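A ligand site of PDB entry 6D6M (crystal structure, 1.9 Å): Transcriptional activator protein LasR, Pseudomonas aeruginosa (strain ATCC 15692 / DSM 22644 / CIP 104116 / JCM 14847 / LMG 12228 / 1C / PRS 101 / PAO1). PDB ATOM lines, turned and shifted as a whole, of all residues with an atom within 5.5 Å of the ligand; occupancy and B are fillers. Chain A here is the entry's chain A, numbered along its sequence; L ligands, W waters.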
ATOM      1  N   LEU A  36      -1.908  24.222 -20.102  1.00  0.00           N
ATOM      2  CA  LEU A  36      -2.557  24.386 -21.399  1.00  0.00           C
ATOM      3  C   LEU A  36      -3.664  25.452 -21.317  1.00  0.00           C
ATOM      4  O   LEU A  36      -4.595  25.350 -20.499  1.00  0.00           O
ATOM      5  CB  LEU A  36      -3.129  23.059 -21.882  1.00  0.00           C
ATOM      6  CG  LEU A  36      -3.473  23.001 -23.368  1.00  0.00           C
ATOM      7  CD1 LEU A  36      -2.189  22.979 -24.218  1.00  0.00           C
ATOM      8  CD2 LEU A  36      -4.323  21.776 -23.675  1.00  0.00           C
ATOM      9  N   GLY A  38      -6.635  27.026 -23.405  1.00  0.00           N
ATOM     10  CA  GLY A  38      -7.461  26.730 -24.578  1.00  0.00           C
ATOM     11  C   GLY A  38      -8.686  27.649 -24.610  1.00  0.00           C
ATOM     12  O   GLY A  38      -9.372  27.817 -23.606  1.00  0.00           O
ATOM     13  N   LEU A  40     -12.090  28.992 -27.154  1.00  0.00           N
ATOM     14  CA  LEU A  40     -12.970  28.918 -28.323  1.00  0.00           C
ATOM     15  C   LEU A  40     -13.803  30.200 -28.466  1.00  0.00           C
ATOM     16  O   LEU A  40     -14.217  30.770 -27.459  1.00  0.00           O
ATOM     17  CB  LEU A  40     -13.931  27.720 -28.195  1.00  0.00           C
ATOM     18  CG  LEU A  40     -13.356  26.301 -28.181  1.00  0.00           C
ATOM     19  CD1 LEU A  40     -14.125  25.394 -27.213  1.00  0.00           C
ATOM     20  CD2 LEU A  40     -13.327  25.704 -29.584  1.00  0.00           C
ATOM     21  N   TYR A  47     -13.646  22.442 -32.981  1.00  0.00           N
ATOM     22  CA  TYR A  47     -12.363  22.948 -32.457  1.00  0.00           C
ATOM     23  C   TYR A  47     -11.494  23.605 -33.519  1.00  0.00           C
ATOM     24  O   TYR A  47     -10.360  23.985 -33.249  1.00  0.00           O
ATOM     25  CB  TYR A  47     -11.600  21.819 -31.763  1.00  0.00           C
ATOM     26  CG  TYR A  47     -12.188  21.446 -30.425  1.00  0.00           C
ATOM     27  CD1 TYR A  47     -13.218  20.516 -30.321  1.00  0.00           C
ATOM     28  CD2 TYR A  47     -11.733  22.068 -29.261  1.00  0.00           C
ATOM     29  CE1 TYR A  47     -13.762  20.191 -29.094  1.00  0.00           C
ATOM     30  CE2 TYR A  47     -12.279  21.760 -28.035  1.00  0.00           C
ATOM     31  CZ  TYR A  47     -13.281  20.820 -27.943  1.00  0.00           C
ATOM     32  OH  TYR A  47     -13.812  20.525 -26.710  1.00  0.00           O
ATOM     33  N   ILE A  52      -5.164  27.407 -28.781  1.00  0.00           N
ATOM     34  CA  ILE A  52      -4.642  26.481 -27.776  1.00  0.00           C
ATOM     35  C   ILE A  52      -3.126  26.649 -27.704  1.00  0.00           C
ATOM     36  O   ILE A  52      -2.427  26.528 -28.703  1.00  0.00           O
ATOM     37  CB  ILE A  52      -4.994  25.018 -28.100  1.00  0.00           C
ATOM     38  CG1 ILE A  52      -6.519  24.850 -28.183  1.00  0.00           C
ATOM     39  CG2 ILE A  52      -4.399  24.079 -27.045  1.00  0.00           C
ATOM     40  CD1 ILE A  52      -6.959  23.586 -28.895  1.00  0.00           C
ATOM     41  N   TYR A  56       2.205  21.457 -22.624  1.00  0.00           N
ATOM     42  CA  TYR A  56       1.875  20.016 -22.630  1.00  0.00           C
ATOM     43  C   TYR A  56       2.723  19.318 -23.699  1.00  0.00           C
ATOM     44  O   TYR A  56       2.935  19.869 -24.778  1.00  0.00           O
ATOM     45  CB  TYR A  56       0.393  19.807 -22.946  1.00  0.00           C
ATOM     46  CG  TYR A  56      -0.574  19.897 -21.755  1.00  0.00           C
ATOM     47  CD1 TYR A  56      -0.226  20.571 -20.571  1.00  0.00           C
ATOM     48  CD2 TYR A  56      -1.831  19.316 -21.831  1.00  0.00           C
ATOM     49  CE1 TYR A  56      -1.120  20.635 -19.510  1.00  0.00           C
ATOM     50  CE2 TYR A  56      -2.735  19.397 -20.782  1.00  0.00           C
ATOM     51  CZ  TYR A  56      -2.376  20.054 -19.624  1.00  0.00           C
ATOM     52  OH  TYR A  56      -3.271  20.107 -18.572  1.00  0.00           O
ATOM     53  N   TRP A  60       1.217  13.823 -26.234  1.00  0.00           N
ATOM     54  CA  TRP A  60      -0.047  13.852 -25.482  1.00  0.00           C
ATOM     55  C   TRP A  60      -1.105  14.721 -26.185  1.00  0.00           C
ATOM     56  O   TRP A  60      -2.270  14.307 -26.300  1.00  0.00           O
ATOM     57  CB  TRP A  60       0.193  14.285 -24.023  1.00  0.00           C
ATOM     58  CG  TRP A  60      -1.066  14.436 -23.200  1.00  0.00           C
ATOM     59  CD1 TRP A  60      -1.490  15.552 -22.554  1.00  0.00           C
ATOM     60  CD2 TRP A  60      -2.060  13.428 -22.946  1.00  0.00           C
ATOM     61  NE1 TRP A  60      -2.684  15.317 -21.899  1.00  0.00           N
ATOM     62  CE2 TRP A  60      -3.058  14.027 -22.124  1.00  0.00           C
ATOM     63  CE3 TRP A  60      -2.204  12.092 -23.311  1.00  0.00           C
ATOM     64  CZ2 TRP A  60      -4.182  13.326 -21.682  1.00  0.00           C
ATOM     65  CZ3 TRP A  60      -3.336  11.390 -22.880  1.00  0.00           C
ATOM     66  CH2 TRP A  60      -4.309  12.014 -22.070  1.00  0.00           C
ATOM     67  N   ARG A  61      -0.713  15.901 -26.643  1.00  0.00           N
ATOM     68  CA  ARG A  61      -1.597  16.739 -27.476  1.00  0.00           C
ATOM     69  C   ARG A  61      -2.174  15.977 -28.688  1.00  0.00           C
ATOM     70  O   ARG A  61      -3.381  16.045 -28.943  1.00  0.00           O
ATOM     71  CB  ARG A  61      -0.871  18.007 -27.965  1.00  0.00           C
ATOM     72  CG  ARG A  61      -0.515  18.993 -26.850  1.00  0.00           C
ATOM     73  CD  ARG A  61      -1.730  19.808 -26.365  1.00  0.00           C
ATOM     74  NE  ARG A  61      -2.478  20.384 -27.468  1.00  0.00           N
ATOM     75  CZ  ARG A  61      -2.091  21.458 -28.171  1.00  0.00           C
ATOM     76  NH1 ARG A  61      -0.966  22.091 -27.871  1.00  0.00           N
ATOM     77  NH2 ARG A  61      -2.835  21.885 -29.168  1.00  0.00           N
ATOM     78  N   TYR A  64      -4.598  12.908 -27.467  1.00  0.00           N
ATOM     79  CA  TYR A  64      -5.858  13.443 -26.957  1.00  0.00           C
ATOM     80  C   TYR A  64      -6.795  13.783 -28.111  1.00  0.00           C
ATOM     81  O   TYR A  64      -7.980  13.445 -28.059  1.00  0.00           O
ATOM     82  CB  TYR A  64      -5.579  14.682 -26.095  1.00  0.00           C
ATOM     83  CG  TYR A  64      -6.776  15.310 -25.386  1.00  0.00           C
ATOM     84  CD1 TYR A  64      -7.691  16.090 -26.081  1.00  0.00           C
ATOM     85  CD2 TYR A  64      -6.953  15.158 -24.002  1.00  0.00           C
ATOM     86  CE1 TYR A  64      -8.767  16.683 -25.432  1.00  0.00           C
ATOM     87  CE2 TYR A  64      -8.028  15.751 -23.353  1.00  0.00           C
ATOM     88  CZ  TYR A  64      -8.926  16.508 -24.079  1.00  0.00           C
ATOM     89  OH  TYR A  64      -9.998  17.108 -23.452  1.00  0.00           O
ATOM     90  N   ASP A  65      -6.249  14.457 -29.122  1.00  0.00           N
ATOM     91  CA  ASP A  65      -6.975  14.780 -30.355  1.00  0.00           C
ATOM     92  C   ASP A  65      -7.424  13.532 -31.115  1.00  0.00           C
ATOM     93  O   ASP A  65      -8.600  13.386 -31.474  1.00  0.00           O
ATOM     94  CB  ASP A  65      -6.117  15.640 -31.275  1.00  0.00           C
ATOM     95  CG  ASP A  65      -6.023  17.090 -30.822  1.00  0.00           C
ATOM     96  OD1 ASP A  65      -6.648  17.470 -29.807  1.00  0.00           O
ATOM     97  OD2 ASP A  65      -5.307  17.864 -31.501  1.00  0.00           O
ATOM     98  N   ASP A  73     -13.130  13.487 -21.424  1.00  0.00           N
ATOM     99  CA  ASP A  73     -12.547  14.329 -20.367  1.00  0.00           C
ATOM    100  C   ASP A  73     -13.617  14.988 -19.489  1.00  0.00           C
ATOM    101  O   ASP A  73     -14.386  15.830 -19.961  1.00  0.00           O
ATOM    102  CB  ASP A  73     -11.693  15.399 -21.067  1.00  0.00           C
ATOM    103  CG  ASP A  73     -10.906  16.275 -20.114  1.00  0.00           C
ATOM    104  OD1 ASP A  73     -11.218  16.362 -18.908  1.00  0.00           O
ATOM    105  OD2 ASP A  73      -9.956  16.908 -20.593  1.00  0.00           O
ATOM    106  N   THR A  75     -13.451  17.224 -17.251  1.00  0.00           N
ATOM    107  CA  THR A  75     -13.229  18.661 -17.029  1.00  0.00           C
ATOM    108  C   THR A  75     -13.855  19.511 -18.128  1.00  0.00           C
ATOM    109  O   THR A  75     -14.223  20.667 -17.884  1.00  0.00           O
ATOM    110  CB  THR A  75     -11.732  19.013 -16.924  1.00  0.00           C
ATOM    111  OG1 THR A  75     -11.104  18.845 -18.201  1.00  0.00           O
ATOM    112  CG2 THR A  75     -11.030  18.138 -15.895  1.00  0.00           C
ATOM    113  N   VAL A  76     -13.953  18.938 -19.329  1.00  0.00           N
ATOM    114  CA  VAL A  76     -14.556  19.638 -20.474  1.00  0.00           C
ATOM    115  C   VAL A  76     -16.046  19.909 -20.236  1.00  0.00           C
ATOM    116  O   VAL A  76     -16.480  21.051 -20.358  1.00  0.00           O
ATOM    117  CB  VAL A  76     -14.337  18.885 -21.814  1.00  0.00           C
ATOM    118  CG1 VAL A  76     -15.174  19.491 -22.928  1.00  0.00           C
ATOM    119  CG2 VAL A  76     -12.857  18.901 -22.196  1.00  0.00           C
ATOM    120  N   CYS A  79     -16.520  22.564 -17.556  1.00  0.00           N
ATOM    121  CA  CYS A  79     -16.313  23.947 -18.022  1.00  0.00           C
ATOM    122  C   CYS A  79     -17.573  24.552 -18.646  1.00  0.00           C
ATOM    123  O   CYS A  79     -17.853  25.729 -18.467  1.00  0.00           O
ATOM    124  CB  CYS A  79     -15.124  24.039 -18.983  1.00  0.00           C
ATOM    125  SG  CYS A  79     -13.503  23.786 -18.225  1.00  0.00           S
ATOM    126  N   THR A  80     -18.335  23.738 -19.376  1.00  0.00           N
ATOM    127  CA  THR A  80     -19.563  24.234 -20.020  1.00  0.00           C
ATOM    128  C   THR A  80     -20.672  24.552 -19.001  1.00  0.00           C
ATOM    129  O   THR A  80     -21.680  25.168 -19.347  1.00  0.00           O
ATOM    130  CB  THR A  80     -20.107  23.227 -21.063  1.00  0.00           C
ATOM    131  OG1 THR A  80     -20.740  22.116 -20.386  1.00  0.00           O
ATOM    132  CG2 THR A  80     -19.013  22.713 -21.969  1.00  0.00           C
ATOM    133  N   TRP A  88      -8.268  17.521 -10.690  1.00  0.00           N
ATOM    134  CA  TRP A  88      -8.127  16.250 -11.399  1.00  0.00           C
ATOM    135  C   TRP A  88      -8.166  15.095 -10.391  1.00  0.00           C
ATOM    136  O   TRP A  88      -7.137  14.767  -9.776  1.00  0.00           O
ATOM    137  CB  TRP A  88      -6.819  16.194 -12.204  1.00  0.00           C
ATOM    138  CG  TRP A  88      -6.635  17.293 -13.181  1.00  0.00           C
ATOM    139  CD1 TRP A  88      -7.559  18.255 -13.551  1.00  0.00           C
ATOM    140  CD2 TRP A  88      -5.471  17.542 -13.968  1.00  0.00           C
ATOM    141  NE1 TRP A  88      -7.019  19.085 -14.502  1.00  0.00           N
ATOM    142  CE2 TRP A  88      -5.744  18.669 -14.785  1.00  0.00           C
ATOM    143  CE3 TRP A  88      -4.217  16.918 -14.058  1.00  0.00           C
ATOM    144  CZ2 TRP A  88      -4.804  19.193 -15.670  1.00  0.00           C
ATOM    145  CZ3 TRP A  88      -3.279  17.436 -14.958  1.00  0.00           C
ATOM    146  CH2 TRP A  88      -3.579  18.574 -15.763  1.00  0.00           C
ATOM    147  N   ILE A  92     -14.041  12.158 -10.595  1.00  0.00           N
ATOM    148  CA  ILE A  92     -14.507  12.737 -11.863  1.00  0.00           C
ATOM    149  C   ILE A  92     -14.467  11.727 -13.024  1.00  0.00           C
ATOM    150  O   ILE A  92     -15.084  11.930 -14.066  1.00  0.00           O
ATOM    151  CB  ILE A  92     -13.857  14.112 -12.213  1.00  0.00           C
ATOM    152  CG1 ILE A  92     -12.337  13.993 -12.475  1.00  0.00           C
ATOM    153  CG2 ILE A  92     -14.165  15.141 -11.145  1.00  0.00           C
ATOM    154  CD1 ILE A  92     -11.629  15.314 -12.751  1.00  0.00           C
ATOM    155  N   TYR A  93     -13.747  10.625 -12.808  1.00  0.00           N
ATOM    156  CA  TYR A  93     -13.675   9.515 -13.762  1.00  0.00           C
ATOM    157  C   TYR A  93     -14.594   8.392 -13.307  1.00  0.00           C
ATOM    158  O   TYR A  93     -14.513   7.945 -12.154  1.00  0.00           O
ATOM    159  CB  TYR A  93     -12.232   9.005 -13.884  1.00  0.00           C
ATOM    160  CG  TYR A  93     -11.198  10.116 -13.939  1.00  0.00           C
ATOM    161  CD1 TYR A  93     -11.023  10.883 -15.082  1.00  0.00           C
ATOM    162  CD2 TYR A  93     -10.389  10.399 -12.834  1.00  0.00           C
ATOM    163  CE1 TYR A  93     -10.098  11.913 -15.135  1.00  0.00           C
ATOM    164  CE2 TYR A  93      -9.442  11.418 -12.886  1.00  0.00           C
ATOM    165  CZ  TYR A  93      -9.310  12.171 -14.030  1.00  0.00           C
ATOM    166  OH  TYR A  93      -8.376  13.172 -14.079  1.00  0.00           O
ATOM    167  N   PHE A 101      -8.832   7.463 -20.136  1.00  0.00           N
ATOM    168  CA  PHE A 101      -8.315   8.833 -20.204  1.00  0.00           C
ATOM    169  C   PHE A 101      -7.392   9.164 -19.039  1.00  0.00           C
ATOM    170  O   PHE A 101      -6.254   9.631 -19.251  1.00  0.00           O
ATOM    171  CB  PHE A 101      -9.455   9.855 -20.293  1.00  0.00           C
ATOM    172  CG  PHE A 101      -9.023  11.282 -20.022  1.00  0.00           C
ATOM    173  CD1 PHE A 101      -8.281  11.997 -20.957  1.00  0.00           C
ATOM    174  CD2 PHE A 101      -9.359  11.911 -18.818  1.00  0.00           C
ATOM    175  CE1 PHE A 101      -7.875  13.300 -20.704  1.00  0.00           C
ATOM    176  CE2 PHE A 101      -8.959  13.220 -18.560  1.00  0.00           C
ATOM    177  CZ  PHE A 101      -8.216  13.906 -19.503  1.00  0.00           C
ATOM    178  N   ALA A 105      -3.352   9.922 -19.346  1.00  0.00           N
ATOM    179  CA  ALA A 105      -2.814  11.189 -18.825  1.00  0.00           C
ATOM    180  C   ALA A 105      -1.707  10.916 -17.793  1.00  0.00           C
ATOM    181  O   ALA A 105      -0.645  11.566 -17.790  1.00  0.00           O
ATOM    182  CB  ALA A 105      -3.925  12.052 -18.216  1.00  0.00           C
ATOM    183  N   LEU A 110       0.973  13.562 -16.463  1.00  0.00           N
ATOM    184  CA  LEU A 110       0.023  14.548 -15.974  1.00  0.00           C
ATOM    185  C   LEU A 110      -0.977  13.859 -15.068  1.00  0.00           C
ATOM    186  O   LEU A 110      -1.997  13.334 -15.523  1.00  0.00           O
ATOM    187  CB  LEU A 110      -0.686  15.242 -17.152  1.00  0.00           C
ATOM    188  CG  LEU A 110       0.282  15.929 -18.114  1.00  0.00           C
ATOM    189  CD1 LEU A 110       0.109  15.431 -19.533  1.00  0.00           C
ATOM    190  CD2 LEU A 110       0.163  17.444 -18.029  1.00  0.00           C
ATOM    191  N   THR A 115      -8.289  22.244 -13.557  1.00  0.00           N
ATOM    192  CA  THR A 115      -8.745  22.906 -14.782  1.00  0.00           C
ATOM    193  C   THR A 115      -9.633  24.074 -14.328  1.00  0.00           C
ATOM    194  O   THR A 115     -10.601  23.877 -13.594  1.00  0.00           O
ATOM    195  CB  THR A 115      -9.500  21.928 -15.701  1.00  0.00           C
ATOM    196  OG1 THR A 115      -8.586  20.957 -16.234  1.00  0.00           O
ATOM    197  CG2 THR A 115     -10.195  22.663 -16.865  1.00  0.00           C
ATOM    198  N   LEU A 125     -15.211  30.703 -24.623  1.00  0.00           N
ATOM    199  CA  LEU A 125     -15.301  29.544 -23.755  1.00  0.00           C
ATOM    200  C   LEU A 125     -13.987  28.774 -23.785  1.00  0.00           C
ATOM    201  O   LEU A 125     -13.492  28.404 -24.842  1.00  0.00           O
ATOM    202  CB  LEU A 125     -16.440  28.619 -24.191  1.00  0.00           C
ATOM    203  CG  LEU A 125     -16.543  27.220 -23.573  1.00  0.00           C
ATOM    204  CD1 LEU A 125     -16.897  27.296 -22.095  1.00  0.00           C
ATOM    205  CD2 LEU A 125     -17.588  26.395 -24.328  1.00  0.00           C
ATOM    206  N   GLY A 126     -13.451  28.475 -22.609  1.00  0.00           N
ATOM    207  CA  GLY A 126     -12.255  27.647 -22.594  1.00  0.00           C
ATOM    208  C   GLY A 126     -11.837  27.233 -21.214  1.00  0.00           C
ATOM    209  O   GLY A 126     -12.666  27.097 -20.305  1.00  0.00           O
ATOM    210  N   ALA A 127     -10.541  27.019 -21.079  1.00  0.00           N
ATOM    211  CA  ALA A 127      -9.981  26.555 -19.812  1.00  0.00           C
ATOM    212  C   ALA A 127      -8.497  26.848 -19.720  1.00  0.00           C
ATOM    213  O   ALA A 127      -7.781  26.803 -20.719  1.00  0.00           O
ATOM    214  CB  ALA A 127     -10.218  25.045 -19.662  1.00  0.00           C
ATOM    215  N   SER A 129      -5.695  24.841 -17.799  1.00  0.00           N
ATOM    216  CA  SER A 129      -5.424  23.585 -17.082  1.00  0.00           C
ATOM    217  C   SER A 129      -3.955  23.568 -16.697  1.00  0.00           C
ATOM    218  O   SER A 129      -3.095  23.956 -17.500  1.00  0.00           O
ATOM    219  CB  SER A 129      -5.771  22.383 -17.954  1.00  0.00           C
ATOM    220  OG  SER A 129      -7.155  22.393 -18.299  1.00  0.00           O
HETATM  221  O1  LIG L   1      -3.497  16.042 -18.871  1.00  0.00           O
HETATM  222  N1  LIG L   1      -4.605  16.416 -19.205  1.00  0.00           N
HETATM  223  O2  LIG L   1      -4.870  16.705 -20.528  1.00  0.00           O
HETATM  224  C1  LIG L   1      -5.648  16.459 -18.277  1.00  0.00           C
HETATM  225  C2  LIG L   1      -5.705  15.488 -17.273  1.00  0.00           C
HETATM  226  C3  LIG L   1      -6.749  15.491 -16.362  1.00  0.00           C
HETATM  227  C4  LIG L   1      -7.767  16.444 -16.436  1.00  0.00           C
HETATM  228  C5  LIG L   1      -7.760  17.435 -17.428  1.00  0.00           C
HETATM  229  C6  LIG L   1      -6.731  17.466 -18.375  1.00  0.00           C
HETATM  230  C7  LIG L   1      -6.747  18.559 -19.390  1.00  0.00           C
HETATM  231  O3  LIG L   1      -5.803  19.341 -19.408  1.00  0.00           O
HETATM  232  N2  LIG L   1      -7.727  18.658 -20.186  1.00  0.00           N
HETATM  233  C8  LIG L   1      -7.879  19.703 -21.170  1.00  0.00           C
HETATM  234  C9  LIG L   1      -7.247  19.413 -22.507  1.00  0.00           C
HETATM  235  C10 LIG L   1      -6.107  18.643 -22.687  1.00  0.00           C
HETATM  236  C11 LIG L   1      -5.611  18.461 -23.983  1.00  0.00           C
HETATM  237 BR1  LIG L   1      -4.104  17.394 -24.209  1.00  0.00          BR
HETATM  238  C12 LIG L   1      -6.157  19.043 -25.123  1.00  0.00           C
HETATM  239  C13 LIG L   1      -7.291  19.830 -24.993  1.00  0.00           C
HETATM  240 BR2  LIG L   1      -8.154  20.686 -26.447  1.00  0.00          BR
HETATM  241  C14 LIG L   1      -7.822  20.126 -23.648  1.00  0.00           C
HETATM  242  O4  LIG L   1      -9.195  20.414 -23.570  1.00  0.00           O
HETATM  243  C15 LIG L   1      -9.313  21.843 -23.409  1.00  0.00           C
HETATM  244  O5  LIG L   1      -8.322  22.571 -23.289  1.00  0.00           O
HETATM  245  C16 LIG L   1     -10.704  22.360 -23.365  1.00  0.00           C
HETATM  246  C17 LIG L   1     -11.034  23.202 -22.324  1.00  0.00           C
HETATM  247  C18 LIG L   1     -11.641  21.967 -24.324  1.00  0.00           C
HETATM  248  C19 LIG L   1     -12.938  22.467 -24.237  1.00  0.00           C
HETATM  249  C20 LIG L   1     -13.260  23.327 -23.185  1.00  0.00           C
HETATM  250  C21 LIG L   1     -12.316  23.697 -22.231  1.00  0.00           C
HETATM  251 BR3  LIG L   1     -14.988  24.024 -22.987  1.00  0.00          BR
HETATM  252  O   HOH W   1      -4.823  18.568 -28.131  1.00  0.00           O
HETATM  253  O   HOH W   2      -7.061  23.600 -20.686  1.00  0.00           O
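The side-chain carboxylate (OD2) of Asp 73 sits at hydrogen-bond distance from a nitrogen (N2) of the ligand.
The side-chain hydroxyl (OH) of Tyr 64 is in hydrogen-bond range of an oxygen (O4) of the ligand, at 3.4 Å.
NE1 of Trp 60 is in hydrogen-bond range of O2 of the ligand (2.9 Å).
OH of Tyr 56 lies within hydrogen-bond range of O3 of the ligand (2.8 Å).
Water W1 lies within hydrogen-bond range of the side-chain carboxylate of Asp 65 (2.7 Å) and the backbone carbonyl oxygen of Arg 61 (3.0 Å).
The side-chain hydroxyl (OG) of Ser 129 sits at hydrogen-bond distance from the side-chain hydroxyl (OG1) of Thr 115, at 2.9 Å.
The backbone NH of Ala 127 lies within hydrogen-bond range of the backbone carbonyl oxygen of Gly 38.
The indole nitrogen of Trp 88 is in hydrogen-bond range of the side-chain hydroxyl of Thr 115 (3.0 Å).
The side-chain carboxylate (OD1) of Asp 73 sits at hydrogen-bond distance from the side-chain hydroxyl (OG1) of Thr 75, 2.6 Å away.
The side-chain carboxylate of Asp 73 lies within hydrogen-bond range of the side-chain hydroxyl of Tyr 64 (2.9 Å).
The backbone NH of Leu 110 is in hydrogen-bond range of the backbone carbonyl oxygen of Ala 105, at 2.9 Å.
O of Ser 129 is in hydrogen-bond range of N of Leu 36 (2.9 Å).
O of Leu 125 sits at hydrogen-bond distance from N of Leu 40 (2.8 Å).
Residues that only touch the ligand: Tyr 47 (3.3 Å), Ala 127 (3.3 Å), Trp 88 (3.4 Å), Ser 129 (3.4 Å), Leu 110 (3.4 Å), Leu 36 (3.6 Å), Leu 125 (3.6 Å), Tyr 93 (3.6 Å), Thr 75 (3.7 Å), Gly 126 (3.7 Å), Phe 101 (3.7 Å), Thr 115 (3.8 Å), Val 76 (3.9 Å), Ile 52 (3.98 Å) and Ala 105 (3.98 Å).
Hydrophobic or aromatic side chains that line the ligand: Leu 36, Tyr 47, Ile 52, Tyr 56, Trp 60, Tyr 64, Val 76, Trp 88, Phe 101, Ala 105, Leu 110, Leu 125 and Ala 127.
19 residues have an atom within 4 Å of the ligand: Leu 36, Tyr 47, Ile 52, Tyr 56, Trp 60, Tyr 64, Asp 73, Thr 75, Val 76, Trp 88, Tyr 93, Phe 101, Ala 105, Leu 110, Thr 115, Leu 125, Gly 126, Ala 127 and Ser 129.
Along chain A the residues within 4 Å of the ligand span positions 36 to 129.
The nearest printed residue that does not touch the ligand is Cys 79 (4.01 Å).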
